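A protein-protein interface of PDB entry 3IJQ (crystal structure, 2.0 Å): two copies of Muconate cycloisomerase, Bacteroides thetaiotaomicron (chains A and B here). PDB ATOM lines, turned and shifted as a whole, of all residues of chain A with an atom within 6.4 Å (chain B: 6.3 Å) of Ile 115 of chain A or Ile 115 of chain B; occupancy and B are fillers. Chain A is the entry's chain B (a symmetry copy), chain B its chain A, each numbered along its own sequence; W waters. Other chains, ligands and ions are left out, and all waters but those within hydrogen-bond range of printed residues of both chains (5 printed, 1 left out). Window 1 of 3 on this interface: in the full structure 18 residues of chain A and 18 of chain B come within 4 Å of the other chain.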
ATOM      1  N   PHE A  73      29.929  33.641 -22.724  1.00  0.00           N
ATOM      2  CA  PHE A  73      28.901  32.916 -21.970  1.00  0.00           C
ATOM      3  C   PHE A  73      28.909  33.199 -20.472  1.00  0.00           C
ATOM      4  O   PHE A  73      27.975  32.833 -19.760  1.00  0.00           O
ATOM      5  CB  PHE A  73      29.029  31.410 -22.214  1.00  0.00           C
ATOM      6  CG  PHE A  73      28.448  30.961 -23.522  1.00  0.00           C
ATOM      7  CD1 PHE A  73      27.096  30.652 -23.623  1.00  0.00           C
ATOM      8  CD2 PHE A  73      29.240  30.893 -24.662  1.00  0.00           C
ATOM      9  CE1 PHE A  73      26.536  30.283 -24.833  1.00  0.00           C
ATOM     10  CE2 PHE A  73      28.690  30.524 -25.892  1.00  0.00           C
ATOM     11  CZ  PHE A  73      27.332  30.218 -25.978  1.00  0.00           C
ATOM     12  N   LEU A  75      27.990  35.464 -18.529  1.00  0.00           N
ATOM     13  CA  LEU A  75      27.170  36.647 -18.338  1.00  0.00           C
ATOM     14  C   LEU A  75      27.083  37.057 -16.877  1.00  0.00           C
ATOM     15  O   LEU A  75      26.934  38.238 -16.575  1.00  0.00           O
ATOM     16  CB  LEU A  75      25.770  36.421 -18.930  1.00  0.00           C
ATOM     17  CG  LEU A  75      25.760  36.101 -20.432  1.00  0.00           C
ATOM     18  CD1 LEU A  75      24.325  35.974 -20.929  1.00  0.00           C
ATOM     19  CD2 LEU A  75      26.498  37.207 -21.203  1.00  0.00           C
ATOM     20  N   HIS A 101      23.461  39.185 -24.780  1.00  0.00           N
ATOM     21  CA  HIS A 101      22.469  38.107 -24.910  1.00  0.00           C
ATOM     22  C   HIS A 101      22.235  37.825 -26.369  1.00  0.00           C
ATOM     23  O   HIS A 101      22.030  36.674 -26.783  1.00  0.00           O
ATOM     24  CB  HIS A 101      21.151  38.482 -24.242  1.00  0.00           C
ATOM     25  CG  HIS A 101      21.244  38.567 -22.752  1.00  0.00           C
ATOM     26  ND1 HIS A 101      20.889  37.524 -21.922  1.00  0.00           N
ATOM     27  CD2 HIS A 101      21.686  39.560 -21.946  1.00  0.00           C
ATOM     28  CE1 HIS A 101      21.109  37.873 -20.668  1.00  0.00           C
ATOM     29  NE2 HIS A 101      21.595  39.103 -20.655  1.00  0.00           N
ATOM     30  N   VAL A 104      25.218  35.734 -27.275  1.00  0.00           N
ATOM     31  CA  VAL A 104      25.103  34.398 -26.694  1.00  0.00           C
ATOM     32  C   VAL A 104      24.012  33.576 -27.376  1.00  0.00           C
ATOM     33  O   VAL A 104      24.204  32.394 -27.671  1.00  0.00           O
ATOM     34  CB  VAL A 104      24.826  34.484 -25.176  1.00  0.00           C
ATOM     35  CG1 VAL A 104      24.400  33.122 -24.627  1.00  0.00           C
ATOM     36  CG2 VAL A 104      26.084  34.954 -24.464  1.00  0.00           C
ATOM     37  N   GLY A 105      22.872  34.205 -27.634  1.00  0.00           N
ATOM     38  CA  GLY A 105      21.776  33.511 -28.285  1.00  0.00           C
ATOM     39  C   GLY A 105      22.169  33.077 -29.681  1.00  0.00           C
ATOM     40  O   GLY A 105      21.845  31.970 -30.128  1.00  0.00           O
ATOM     41  N   LEU A 108      24.272  30.108 -29.567  1.00  0.00           N
ATOM     42  CA  LEU A 108      23.535  28.913 -29.167  1.00  0.00           C
ATOM     43  C   LEU A 108      22.545  28.513 -30.240  1.00  0.00           C
ATOM     44  O   LEU A 108      22.001  27.415 -30.206  1.00  0.00           O
ATOM     45  CB  LEU A 108      22.767  29.153 -27.867  1.00  0.00           C
ATOM     46  CG  LEU A 108      23.535  29.016 -26.559  1.00  0.00           C
ATOM     47  CD1 LEU A 108      22.564  29.166 -25.406  1.00  0.00           C
ATOM     48  CD2 LEU A 108      24.211  27.652 -26.495  1.00  0.00           C
ATOM     49  N   ALA A 110      19.626  30.102 -30.827  1.00  0.00           N
ATOM     50  CA  ALA A 110      18.287  30.152 -30.275  1.00  0.00           C
ATOM     51  C   ALA A 110      17.870  31.508 -29.740  1.00  0.00           C
ATOM     52  O   ALA A 110      18.698  32.267 -29.241  1.00  0.00           O
ATOM     53  CB  ALA A 110      18.159  29.112 -29.158  1.00  0.00           C
ATOM     54  N   PRO A 111      16.568  31.824 -29.838  1.00  0.00           N
ATOM     55  CA  PRO A 111      15.989  33.083 -29.355  1.00  0.00           C
ATOM     56  C   PRO A 111      15.990  32.934 -27.836  1.00  0.00           C
ATOM     57  O   PRO A 111      15.876  31.805 -27.333  1.00  0.00           O
ATOM     58  CB  PRO A 111      14.558  33.051 -29.901  1.00  0.00           C
ATOM     59  CG  PRO A 111      14.597  32.029 -30.998  1.00  0.00           C
ATOM     60  CD  PRO A 111      15.548  31.005 -30.512  1.00  0.00           C
ATOM     61  N   TRP A 112      16.107  34.033 -27.099  1.00  0.00           N
ATOM     62  CA  TRP A 112      16.120  33.910 -25.647  1.00  0.00           C
ATOM     63  C   TRP A 112      14.811  33.420 -25.035  1.00  0.00           C
ATOM     64  O   TRP A 112      14.828  32.830 -23.960  1.00  0.00           O
ATOM     65  CB  TRP A 112      16.571  35.223 -24.978  1.00  0.00           C
ATOM     66  CG  TRP A 112      18.056  35.258 -24.854  1.00  0.00           C
ATOM     67  CD1 TRP A 112      18.946  35.702 -25.794  1.00  0.00           C
ATOM     68  CD2 TRP A 112      18.838  34.655 -23.815  1.00  0.00           C
ATOM     69  NE1 TRP A 112      20.234  35.398 -25.406  1.00  0.00           N
ATOM     70  CE2 TRP A 112      20.194  34.756 -24.198  1.00  0.00           C
ATOM     71  CE3 TRP A 112      18.522  34.029 -22.600  1.00  0.00           C
ATOM     72  CZ2 TRP A 112      21.232  34.257 -23.412  1.00  0.00           C
ATOM     73  CZ3 TRP A 112      19.551  33.537 -21.820  1.00  0.00           C
ATOM     74  CH2 TRP A 112      20.894  33.653 -22.229  1.00  0.00           C
ATOM     75  N   TYR A 113      13.681  33.651 -25.697  1.00  0.00           N
ATOM     76  CA  TYR A 113      12.413  33.171 -25.147  1.00  0.00           C
ATOM     77  C   TYR A 113      12.450  31.636 -25.103  1.00  0.00           C
ATOM     78  O   TYR A 113      11.798  30.999 -24.269  1.00  0.00           O
ATOM     79  CB  TYR A 113      11.215  33.658 -25.992  1.00  0.00           C
ATOM     80  CG  TYR A 113      10.941  32.879 -27.270  1.00  0.00           C
ATOM     81  CD1 TYR A 113      10.369  31.605 -27.232  1.00  0.00           C
ATOM     82  CD2 TYR A 113      11.300  33.398 -28.514  1.00  0.00           C
ATOM     83  CE1 TYR A 113      10.175  30.863 -28.400  1.00  0.00           C
ATOM     84  CE2 TYR A 113      11.109  32.668 -29.684  1.00  0.00           C
ATOM     85  CZ  TYR A 113      10.557  31.402 -29.620  1.00  0.00           C
ATOM     86  OH  TYR A 113      10.459  30.648 -30.769  1.00  0.00           O
ATOM     87  N   LYS A 114      13.235  31.058 -26.003  1.00  0.00           N
ATOM     88  CA  LYS A 114      13.368  29.612 -26.116  1.00  0.00           C
ATOM     89  C   LYS A 114      14.349  29.104 -25.067  1.00  0.00           C
ATOM     90  O   LYS A 114      14.090  28.115 -24.376  1.00  0.00           O
ATOM     91  CB  LYS A 114      13.833  29.269 -27.532  1.00  0.00           C
ATOM     92  CG  LYS A 114      13.757  27.802 -27.904  1.00  0.00           C
ATOM     93  CD  LYS A 114      14.051  27.596 -29.390  1.00  0.00           C
ATOM     94  CE  LYS A 114      14.078  26.116 -29.743  1.00  0.00           C
ATOM     95  NZ  LYS A 114      14.461  25.846 -31.166  1.00  0.00           N
ATOM     96  N   ILE A 115      15.475  29.797 -24.942  1.00  0.00           N
ATOM     97  CA  ILE A 115      16.489  29.441 -23.958  1.00  0.00           C
ATOM     98  C   ILE A 115      15.854  29.488 -22.561  1.00  0.00           C
ATOM     99  O   ILE A 115      16.190  28.686 -21.682  1.00  0.00           O
ATOM    100  CB  ILE A 115      17.676  30.436 -24.027  1.00  0.00           C
ATOM    101  CG1 ILE A 115      18.382  30.276 -25.381  1.00  0.00           C
ATOM    102  CG2 ILE A 115      18.639  30.208 -22.870  1.00  0.00           C
ATOM    103  CD1 ILE A 115      19.487  31.262 -25.636  1.00  0.00           C
ATOM    104  N   TRP A 116      14.929  30.425 -22.373  1.00  0.00           N
ATOM    105  CA  TRP A 116      14.223  30.603 -21.105  1.00  0.00           C
ATOM    106  C   TRP A 116      13.044  29.642 -20.909  1.00  0.00           C
ATOM    107  O   TRP A 116      12.406  29.637 -19.846  1.00  0.00           O
ATOM    108  CB  TRP A 116      13.716  32.037 -20.982  1.00  0.00           C
ATOM    109  CG  TRP A 116      14.775  33.048 -20.645  1.00  0.00           C
ATOM    110  CD1 TRP A 116      15.895  32.849 -19.893  1.00  0.00           C
ATOM    111  CD2 TRP A 116      14.743  34.445 -20.961  1.00  0.00           C
ATOM    112  NE1 TRP A 116      16.564  34.047 -19.713  1.00  0.00           N
ATOM    113  CE2 TRP A 116      15.876  35.038 -20.362  1.00  0.00           C
ATOM    114  CE3 TRP A 116      13.864  35.253 -21.697  1.00  0.00           C
ATOM    115  CZ2 TRP A 116      16.154  36.402 -20.473  1.00  0.00           C
ATOM    116  CZ3 TRP A 116      14.144  36.627 -21.806  1.00  0.00           C
ATOM    117  CH2 TRP A 116      15.276  37.178 -21.198  1.00  0.00           C
ATOM    118  N   GLY A 117      12.748  28.858 -21.943  1.00  0.00           N
ATOM    119  CA  GLY A 117      11.675  27.876 -21.878  1.00  0.00           C
ATOM    120  C   GLY A 117      10.250  28.395 -21.898  1.00  0.00           C
ATOM    121  O   GLY A 117       9.367  27.816 -21.256  1.00  0.00           O
ATOM    122  N   LEU A 118      10.007  29.469 -22.647  1.00  0.00           N
ATOM    123  CA  LEU A 118       8.674  30.062 -22.716  1.00  0.00           C
ATOM    124  C   LEU A 118       7.988  29.751 -24.034  1.00  0.00           C
ATOM    125  O   LEU A 118       8.641  29.474 -25.040  1.00  0.00           O
ATOM    126  CB  LEU A 118       8.761  31.586 -22.540  1.00  0.00           C
ATOM    127  CG  LEU A 118       9.548  32.089 -21.323  1.00  0.00           C
ATOM    128  CD1 LEU A 118       9.639  33.628 -21.347  1.00  0.00           C
ATOM    129  CD2 LEU A 118       8.860  31.623 -20.048  1.00  0.00           C
ATOM    130  N   ARG A 261      19.114  40.091 -18.206  1.00  0.00           N
ATOM    131  CA  ARG A 261      19.426  39.216 -17.085  1.00  0.00           C
ATOM    132  C   ARG A 261      18.733  39.651 -15.794  1.00  0.00           C
ATOM    133  O   ARG A 261      18.073  38.840 -15.142  1.00  0.00           O
ATOM    134  CB  ARG A 261      20.939  39.137 -16.884  1.00  0.00           C
ATOM    135  CG  ARG A 261      21.386  37.950 -16.045  1.00  0.00           C
ATOM    136  CD  ARG A 261      22.892  37.813 -16.078  1.00  0.00           C
ATOM    137  NE  ARG A 261      23.374  36.730 -15.228  1.00  0.00           N
ATOM    138  CZ  ARG A 261      23.272  35.440 -15.524  1.00  0.00           C
ATOM    139  NH1 ARG A 261      22.700  35.057 -16.656  1.00  0.00           N
ATOM    140  NH2 ARG A 261      23.745  34.532 -14.682  1.00  0.00           N
ATOM    141  N   GLY A 332      19.026  34.860 -30.406  1.00  0.00           N
ATOM    142  CA  GLY A 332      19.434  36.047 -29.672  1.00  0.00           C
ATOM    143  C   GLY A 332      18.211  36.846 -29.257  1.00  0.00           C
ATOM    144  O   GLY A 332      17.257  36.293 -28.687  1.00  0.00           O
ATOM    145  N   PHE B  73      11.516  22.401 -25.617  1.00  0.00           N
ATOM    146  CA  PHE B  73      11.930  23.691 -25.077  1.00  0.00           C
ATOM    147  C   PHE B  73      10.892  24.389 -24.217  1.00  0.00           C
ATOM    148  O   PHE B  73      11.222  25.270 -23.423  1.00  0.00           O
ATOM    149  CB  PHE B  73      12.369  24.603 -26.219  1.00  0.00           C
ATOM    150  CG  PHE B  73      13.685  24.211 -26.810  1.00  0.00           C
ATOM    151  CD1 PHE B  73      14.869  24.705 -26.279  1.00  0.00           C
ATOM    152  CD2 PHE B  73      13.746  23.294 -27.858  1.00  0.00           C
ATOM    153  CE1 PHE B  73      16.099  24.289 -26.780  1.00  0.00           C
ATOM    154  CE2 PHE B  73      14.971  22.872 -28.363  1.00  0.00           C
ATOM    155  CZ  PHE B  73      16.151  23.373 -27.820  1.00  0.00           C
ATOM    156  N   LEU B  75       9.676  24.352 -21.442  1.00  0.00           N
ATOM    157  CA  LEU B  75       9.842  23.895 -20.072  1.00  0.00           C
ATOM    158  C   LEU B  75       8.862  24.521 -19.097  1.00  0.00           C
ATOM    159  O   LEU B  75       8.447  23.872 -18.143  1.00  0.00           O
ATOM    160  CB  LEU B  75      11.285  24.128 -19.601  1.00  0.00           C
ATOM    161  CG  LEU B  75      12.341  23.320 -20.376  1.00  0.00           C
ATOM    162  CD1 LEU B  75      13.693  23.431 -19.681  1.00  0.00           C
ATOM    163  CD2 LEU B  75      11.910  21.851 -20.456  1.00  0.00           C
ATOM    164  N   HIS B 101      15.738  18.923 -18.896  1.00  0.00           N
ATOM    165  CA  HIS B 101      16.844  19.869 -18.985  1.00  0.00           C
ATOM    166  C   HIS B 101      18.017  19.219 -19.701  1.00  0.00           C
ATOM    167  O   HIS B 101      18.697  19.853 -20.510  1.00  0.00           O
ATOM    168  CB  HIS B 101      17.254  20.330 -17.587  1.00  0.00           C
ATOM    169  CG  HIS B 101      16.292  21.303 -16.980  1.00  0.00           C
ATOM    170  ND1 HIS B 101      16.391  22.666 -17.171  1.00  0.00           N
ATOM    171  CD2 HIS B 101      15.189  21.109 -16.219  1.00  0.00           C
ATOM    172  CE1 HIS B 101      15.392  23.266 -16.551  1.00  0.00           C
ATOM    173  NE2 HIS B 101      14.647  22.345 -15.967  1.00  0.00           N
ATOM    174  N   VAL B 104      17.098  19.265 -23.430  1.00  0.00           N
ATOM    175  CA  VAL B 104      17.193  20.627 -23.955  1.00  0.00           C
ATOM    176  C   VAL B 104      18.638  21.108 -24.056  1.00  0.00           C
ATOM    177  O   VAL B 104      19.017  21.770 -25.029  1.00  0.00           O
ATOM    178  CB  VAL B 104      16.384  21.613 -23.080  1.00  0.00           C
ATOM    179  CG1 VAL B 104      16.712  23.070 -23.452  1.00  0.00           C
ATOM    180  CG2 VAL B 104      14.900  21.351 -23.281  1.00  0.00           C
ATOM    181  N   GLY B 105      19.441  20.780 -23.053  1.00  0.00           N
ATOM    182  CA  GLY B 105      20.831  21.191 -23.081  1.00  0.00           C
ATOM    183  C   GLY B 105      21.537  20.529 -24.249  1.00  0.00           C
ATOM    184  O   GLY B 105      22.322  21.158 -24.964  1.00  0.00           O
ATOM    185  N   LEU B 108      20.673  22.102 -27.433  1.00  0.00           N
ATOM    186  CA  LEU B 108      21.339  23.398 -27.564  1.00  0.00           C
ATOM    187  C   LEU B 108      22.840  23.223 -27.687  1.00  0.00           C
ATOM    188  O   LEU B 108      23.536  24.128 -28.137  1.00  0.00           O
ATOM    189  CB  LEU B 108      21.054  24.292 -26.358  1.00  0.00           C
ATOM    190  CG  LEU B 108      19.685  24.963 -26.311  1.00  0.00           C
ATOM    191  CD1 LEU B 108      19.586  25.791 -25.050  1.00  0.00           C
ATOM    192  CD2 LEU B 108      19.499  25.847 -27.539  1.00  0.00           C
ATOM    193  N   ALA B 110      24.928  22.623 -25.054  1.00  0.00           N
ATOM    194  CA  ALA B 110      25.587  23.313 -23.966  1.00  0.00           C
ATOM    195  C   ALA B 110      25.160  22.808 -22.596  1.00  0.00           C
ATOM    196  O   ALA B 110      24.041  22.333 -22.423  1.00  0.00           O
ATOM    197  CB  ALA B 110      25.309  24.807 -24.068  1.00  0.00           C
ATOM    198  N   PRO B 111      26.068  22.889 -21.608  1.00  0.00           N
ATOM    199  CA  PRO B 111      25.794  22.453 -20.232  1.00  0.00           C
ATOM    200  C   PRO B 111      24.893  23.521 -19.637  1.00  0.00           C
ATOM    201  O   PRO B 111      24.935  24.674 -20.076  1.00  0.00           O
ATOM    202  CB  PRO B 111      27.177  22.476 -19.571  1.00  0.00           C
ATOM    203  CG  PRO B 111      28.141  22.386 -20.729  1.00  0.00           C
ATOM    204  CD  PRO B 111      27.488  23.235 -21.776  1.00  0.00           C
ATOM    205  N   TRP B 112      24.085  23.178 -18.638  1.00  0.00           N
ATOM    206  CA  TRP B 112      23.233  24.206 -18.064  1.00  0.00           C
ATOM    207  C   TRP B 112      23.953  25.303 -17.290  1.00  0.00           C
ATOM    208  O   TRP B 112      23.468  26.425 -17.241  1.00  0.00           O
ATOM    209  CB  TRP B 112      22.117  23.590 -17.223  1.00  0.00           C
ATOM    210  CG  TRP B 112      20.959  23.232 -18.094  1.00  0.00           C
ATOM    211  CD1 TRP B 112      20.722  22.029 -18.692  1.00  0.00           C
ATOM    212  CD2 TRP B 112      19.931  24.121 -18.556  1.00  0.00           C
ATOM    213  NE1 TRP B 112      19.609  22.115 -19.501  1.00  0.00           N
ATOM    214  CE2 TRP B 112      19.107  23.387 -19.433  1.00  0.00           C
ATOM    215  CE3 TRP B 112      19.633  25.470 -18.315  1.00  0.00           C
ATOM    216  CZ2 TRP B 112      18.002  23.952 -20.073  1.00  0.00           C
ATOM    217  CZ3 TRP B 112      18.537  26.033 -18.950  1.00  0.00           C
ATOM    218  CH2 TRP B 112      17.732  25.272 -19.822  1.00  0.00           C
ATOM    219  N   TYR B 113      25.108  25.014 -16.699  1.00  0.00           N
ATOM    220  CA  TYR B 113      25.813  26.068 -15.979  1.00  0.00           C
ATOM    221  C   TYR B 113      26.169  27.183 -16.968  1.00  0.00           C
ATOM    222  O   TYR B 113      26.204  28.368 -16.615  1.00  0.00           O
ATOM    223  CB  TYR B 113      27.090  25.526 -15.310  1.00  0.00           C
ATOM    224  CG  TYR B 113      28.268  25.284 -16.238  1.00  0.00           C
ATOM    225  CD1 TYR B 113      29.023  26.350 -16.732  1.00  0.00           C
ATOM    226  CD2 TYR B 113      28.628  23.988 -16.625  1.00  0.00           C
ATOM    227  CE1 TYR B 113      30.094  26.141 -17.588  1.00  0.00           C
ATOM    228  CE2 TYR B 113      29.709  23.765 -17.485  1.00  0.00           C
ATOM    229  CZ  TYR B 113      30.429  24.851 -17.964  1.00  0.00           C
ATOM    230  OH  TYR B 113      31.449  24.664 -18.860  1.00  0.00           O
ATOM    231  N   LYS B 114      26.425  26.784 -18.210  1.00  0.00           N
ATOM    232  CA  LYS B 114      26.803  27.705 -19.272  1.00  0.00           C
ATOM    233  C   LYS B 114      25.568  28.427 -19.795  1.00  0.00           C
ATOM    234  O   LYS B 114      25.588  29.636 -20.015  1.00  0.00           O
ATOM    235  CB  LYS B 114      27.507  26.924 -20.390  1.00  0.00           C
ATOM    236  CG  LYS B 114      28.168  27.784 -21.455  1.00  0.00           C
ATOM    237  CD  LYS B 114      28.957  26.935 -22.450  1.00  0.00           C
ATOM    238  CE  LYS B 114      29.517  27.795 -23.582  1.00  0.00           C
ATOM    239  NZ  LYS B 114      30.211  27.018 -24.657  1.00  0.00           N
ATOM    240  N   ILE B 115      24.483  27.685 -19.986  1.00  0.00           N
ATOM    241  CA  ILE B 115      23.246  28.288 -20.452  1.00  0.00           C
ATOM    242  C   ILE B 115      22.814  29.343 -19.429  1.00  0.00           C
ATOM    243  O   ILE B 115      22.317  30.425 -19.790  1.00  0.00           O
ATOM    244  CB  ILE B 115      22.147  27.211 -20.615  1.00  0.00           C
ATOM    245  CG1 ILE B 115      22.481  26.336 -21.831  1.00  0.00           C
ATOM    246  CG2 ILE B 115      20.769  27.867 -20.742  1.00  0.00           C
ATOM    247  CD1 ILE B 115      21.610  25.103 -21.986  1.00  0.00           C
ATOM    248  N   TRP B 116      23.028  29.034 -18.153  1.00  0.00           N
ATOM    249  CA  TRP B 116      22.671  29.949 -17.075  1.00  0.00           C
ATOM    250  C   TRP B 116      23.709  31.061 -16.905  1.00  0.00           C
ATOM    251  O   TRP B 116      23.561  31.911 -16.038  1.00  0.00           O
ATOM    252  CB  TRP B 116      22.519  29.197 -15.750  1.00  0.00           C
ATOM    253  CG  TRP B 116      21.245  28.373 -15.608  1.00  0.00           C
ATOM    254  CD1 TRP B 116      19.994  28.679 -16.085  1.00  0.00           C
ATOM    255  CD2 TRP B 116      21.098  27.160 -14.853  1.00  0.00           C
ATOM    256  NE1 TRP B 116      19.084  27.734 -15.667  1.00  0.00           N
ATOM    257  CE2 TRP B 116      19.734  26.792 -14.910  1.00  0.00           C
ATOM    258  CE3 TRP B 116      21.992  26.350 -14.131  1.00  0.00           C
ATOM    259  CZ2 TRP B 116      19.236  25.644 -14.271  1.00  0.00           C
ATOM    260  CZ3 TRP B 116      21.494  25.203 -13.489  1.00  0.00           C
ATOM    261  CH2 TRP B 116      20.132  24.866 -13.566  1.00  0.00           C
ATOM    262  N   GLY B 117      24.761  31.034 -17.723  1.00  0.00           N
ATOM    263  CA  GLY B 117      25.799  32.058 -17.669  1.00  0.00           C
ATOM    264  C   GLY B 117      26.759  32.060 -16.487  1.00  0.00           C
ATOM    265  O   GLY B 117      27.334  33.101 -16.152  1.00  0.00           O
ATOM    266  N   LEU B 118      26.964  30.904 -15.862  1.00  0.00           N
ATOM    267  CA  LEU B 118      27.847  30.813 -14.695  1.00  0.00           C
ATOM    268  C   LEU B 118      29.286  30.441 -15.052  1.00  0.00           C
ATOM    269  O   LEU B 118      29.548  29.932 -16.137  1.00  0.00           O
ATOM    270  CB  LEU B 118      27.285  29.783 -13.711  1.00  0.00           C
ATOM    271  CG  LEU B 118      25.824  29.989 -13.299  1.00  0.00           C
ATOM    272  CD1 LEU B 118      25.321  28.787 -12.512  1.00  0.00           C
ATOM    273  CD2 LEU B 118      25.710  31.262 -12.474  1.00  0.00           C
ATOM    274  N   ARG B 261      14.648  23.673 -12.749  1.00  0.00           N
ATOM    275  CA  ARG B 261      13.985  24.933 -13.058  1.00  0.00           C
ATOM    276  C   ARG B 261      13.555  25.669 -11.804  1.00  0.00           C
ATOM    277  O   ARG B 261      13.823  26.870 -11.665  1.00  0.00           O
ATOM    278  CB  ARG B 261      12.784  24.711 -13.983  1.00  0.00           C
ATOM    279  CG  ARG B 261      12.215  26.010 -14.565  1.00  0.00           C
ATOM    280  CD  ARG B 261      11.123  25.756 -15.596  1.00  0.00           C
ATOM    281  NE  ARG B 261      10.605  27.003 -16.165  1.00  0.00           N
ATOM    282  CZ  ARG B 261      11.188  27.692 -17.147  1.00  0.00           C
ATOM    283  NH1 ARG B 261      12.320  27.260 -17.693  1.00  0.00           N
ATOM    284  NH2 ARG B 261      10.638  28.823 -17.582  1.00  0.00           N
ATOM    285  N   GLY B 332      23.688  19.512 -21.513  1.00  0.00           N
ATOM    286  CA  GLY B 332      22.646  19.088 -20.598  1.00  0.00           C
ATOM    287  C   GLY B 332      23.117  19.106 -19.162  1.00  0.00           C
ATOM    288  O   GLY B 332      23.709  20.095 -18.704  1.00  0.00           O
HETATM  289  O   HOH W   1      29.150  30.282 -18.807  1.00  0.00           O
HETATM  290  O   HOH W   2      25.268  32.385 -20.881  1.00  0.00           O
HETATM  291  O   HOH W   3      10.278  27.483 -25.475  1.00  0.00           O
HETATM  292  O   HOH W   4      23.009  33.089 -19.219  1.00  0.00           O
HETATM  293  O   HOH W   5      14.470  27.023 -20.103  1.00  0.00           O
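Of the 17 printed residues of chain A, 9 touch a printed residue of chain B. Printed residues of chain A that touch a printed residue of chain B: Phe 73, Leu 75, Leu 108, Ala 110, Lys 114, Ile 115, Trp 116, Gly 117 and Arg 261. Among the printed residues, no Asp or Glu carboxylate lies within 4 Å of a Lys or Arg side-chain nitrogen of the other chain.
A ring nitrogen (NE2) of His 101 of chain B is in hydrogen-bond range of the backbone NH (N) of Arg 261 of chain B (3.5 Å). The backbone NH of Ala 110 of chain B sits at hydrogen-bond distance from the backbone carbonyl oxygen of Gly 105 of chain B (3.0 Å). O of Ala 110 of chain B lies within hydrogen-bond range of N of Gly 332 of chain B, 3.0 Å away. The backbone carbonyl oxygen (O) of Gly 105 of chain A sits at hydrogen-bond distance from the backbone NH (N) of Ala 110 of chain A. The backbone carbonyl oxygen (O) of Ala 110 of chain A is in hydrogen-bond range of the backbone NH (N) of Gly 332 of chain A (2.9 Å).
The backbone carbonyl oxygen of Gly 117 of chain A is in hydrogen-bond range of the backbone NH of Leu 75 of chain B (3.5 Å). O of Trp 116 of chain B sits at hydrogen-bond distance from NH2 of Arg 261 of chain A. The backbone NH (N) of Leu 75 of chain A lies within hydrogen-bond range of the backbone carbonyl oxygen (O) of Gly 117 of chain B (3.4 Å). The guanidinium group of Arg 261 of chain B is in hydrogen-bond range of the backbone carbonyl oxygen of Trp 116 of chain A.
Phe 73 of chain A touches Lys 114 of chain B, and with the chains exchanged Lys 114 of chain A touches Phe 73 of chain B. Phe 73 of chain A touches Gly 117 of chain B, and with the chains exchanged Gly 117 of chain A touches Phe 73 of chain B. Leu 75 of chain A touches Gly 117 of chain B, and with the chains exchanged Gly 117 of chain A touches Leu 75 of chain B. Leu 108 of chain A touches Ala 110 of chain B, and with the chains exchanged Ala 110 of chain A touches Leu 108 of chain B. Positions printed for both chains: 73, 75, 101, 104, 105, 108, 110, 111, 112, 113, 114, 115, 116, 117, 118, 261 and 332.
Of the printed residues of chain B, Lys 114 of chain A touches Phe 73. Ile 115 of chain A touches just one residue of chain B: Ile 115. Of the printed residues of chain B, Arg 261 of chain A touches Trp 116 (3.0 Å). Printed residues of chain A within 4 Å of Leu 75 of chain B: Gly 117. Of the printed residues of chain A, Leu 108 of chain B touches Leu 108 and Ala 110. Printed residues of chain A within 4 Å of Lys 114 of chain B: Phe 73. The nearest residue of chain B that does not touch Ile 115 of chain A is Trp 112 of chain B (4.2 Å). The nearest residue of chain A that does not touch Ile 115 of chain B is Trp 112 of chain A (4.3 Å). The nearest printed residue of chain A that does not touch Ala 110 of chain B is Phe 73 of chain A (5.7 Å).
Water W3 lies within hydrogen-bond range of O of Leu 118 of chain A (2.6 Å) and O of Phe 73 of chain B (3.2 Å). Water W1 bridges O of Leu 118 of chain B (2.7 Å) and O of Phe 73 of chain A (3.0 Å). Water W4 lies within hydrogen-bond range of the backbone carbonyl oxygen of Ile 115 of chain B (2.8 Å), the backbone NH of Gly 117 of chain B (3.1 Å), the guanidinium group of Arg 261 of chain A (3.2 Å) and the backbone carbonyl oxygen of Trp 116 of chain B (3.4 Å). Water W5 lies within hydrogen-bond range of the backbone carbonyl oxygen (O) of Ile 115 of chain A (2.9 Å), the backbone NH (N) of Gly 117 of chain A (3.1 Å), the guanidinium group (NH1) of Arg 261 of chain B (3.2 Å) and the backbone carbonyl oxygen (O) of Trp 116 of chain A (3.3 Å). Water W2 lies within hydrogen-bond range of O of Lys 114 of chain B (2.9 Å), O of Phe 73 of chain A (3.0 Å) and N of Gly 117 of chain B (3.5 Å).
Among the printed residues, pairs that only touch across the chains: Gly 117 of chain A with Phe 73 of chain B, Phe 73 of chain A with Gly 117 of chain B, Phe 73 of chain A with Lys 114 of chain B, Lys 114 of chain A with Phe 73 of chain B, Ile 115 of chain A with Ile 115 of chain B, Ala 110 of chain A with Leu 108 of chain B, Leu 108 of chain A with Ala 110 of chain B and Leu 108 of chain A with Leu 108 of chain B.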
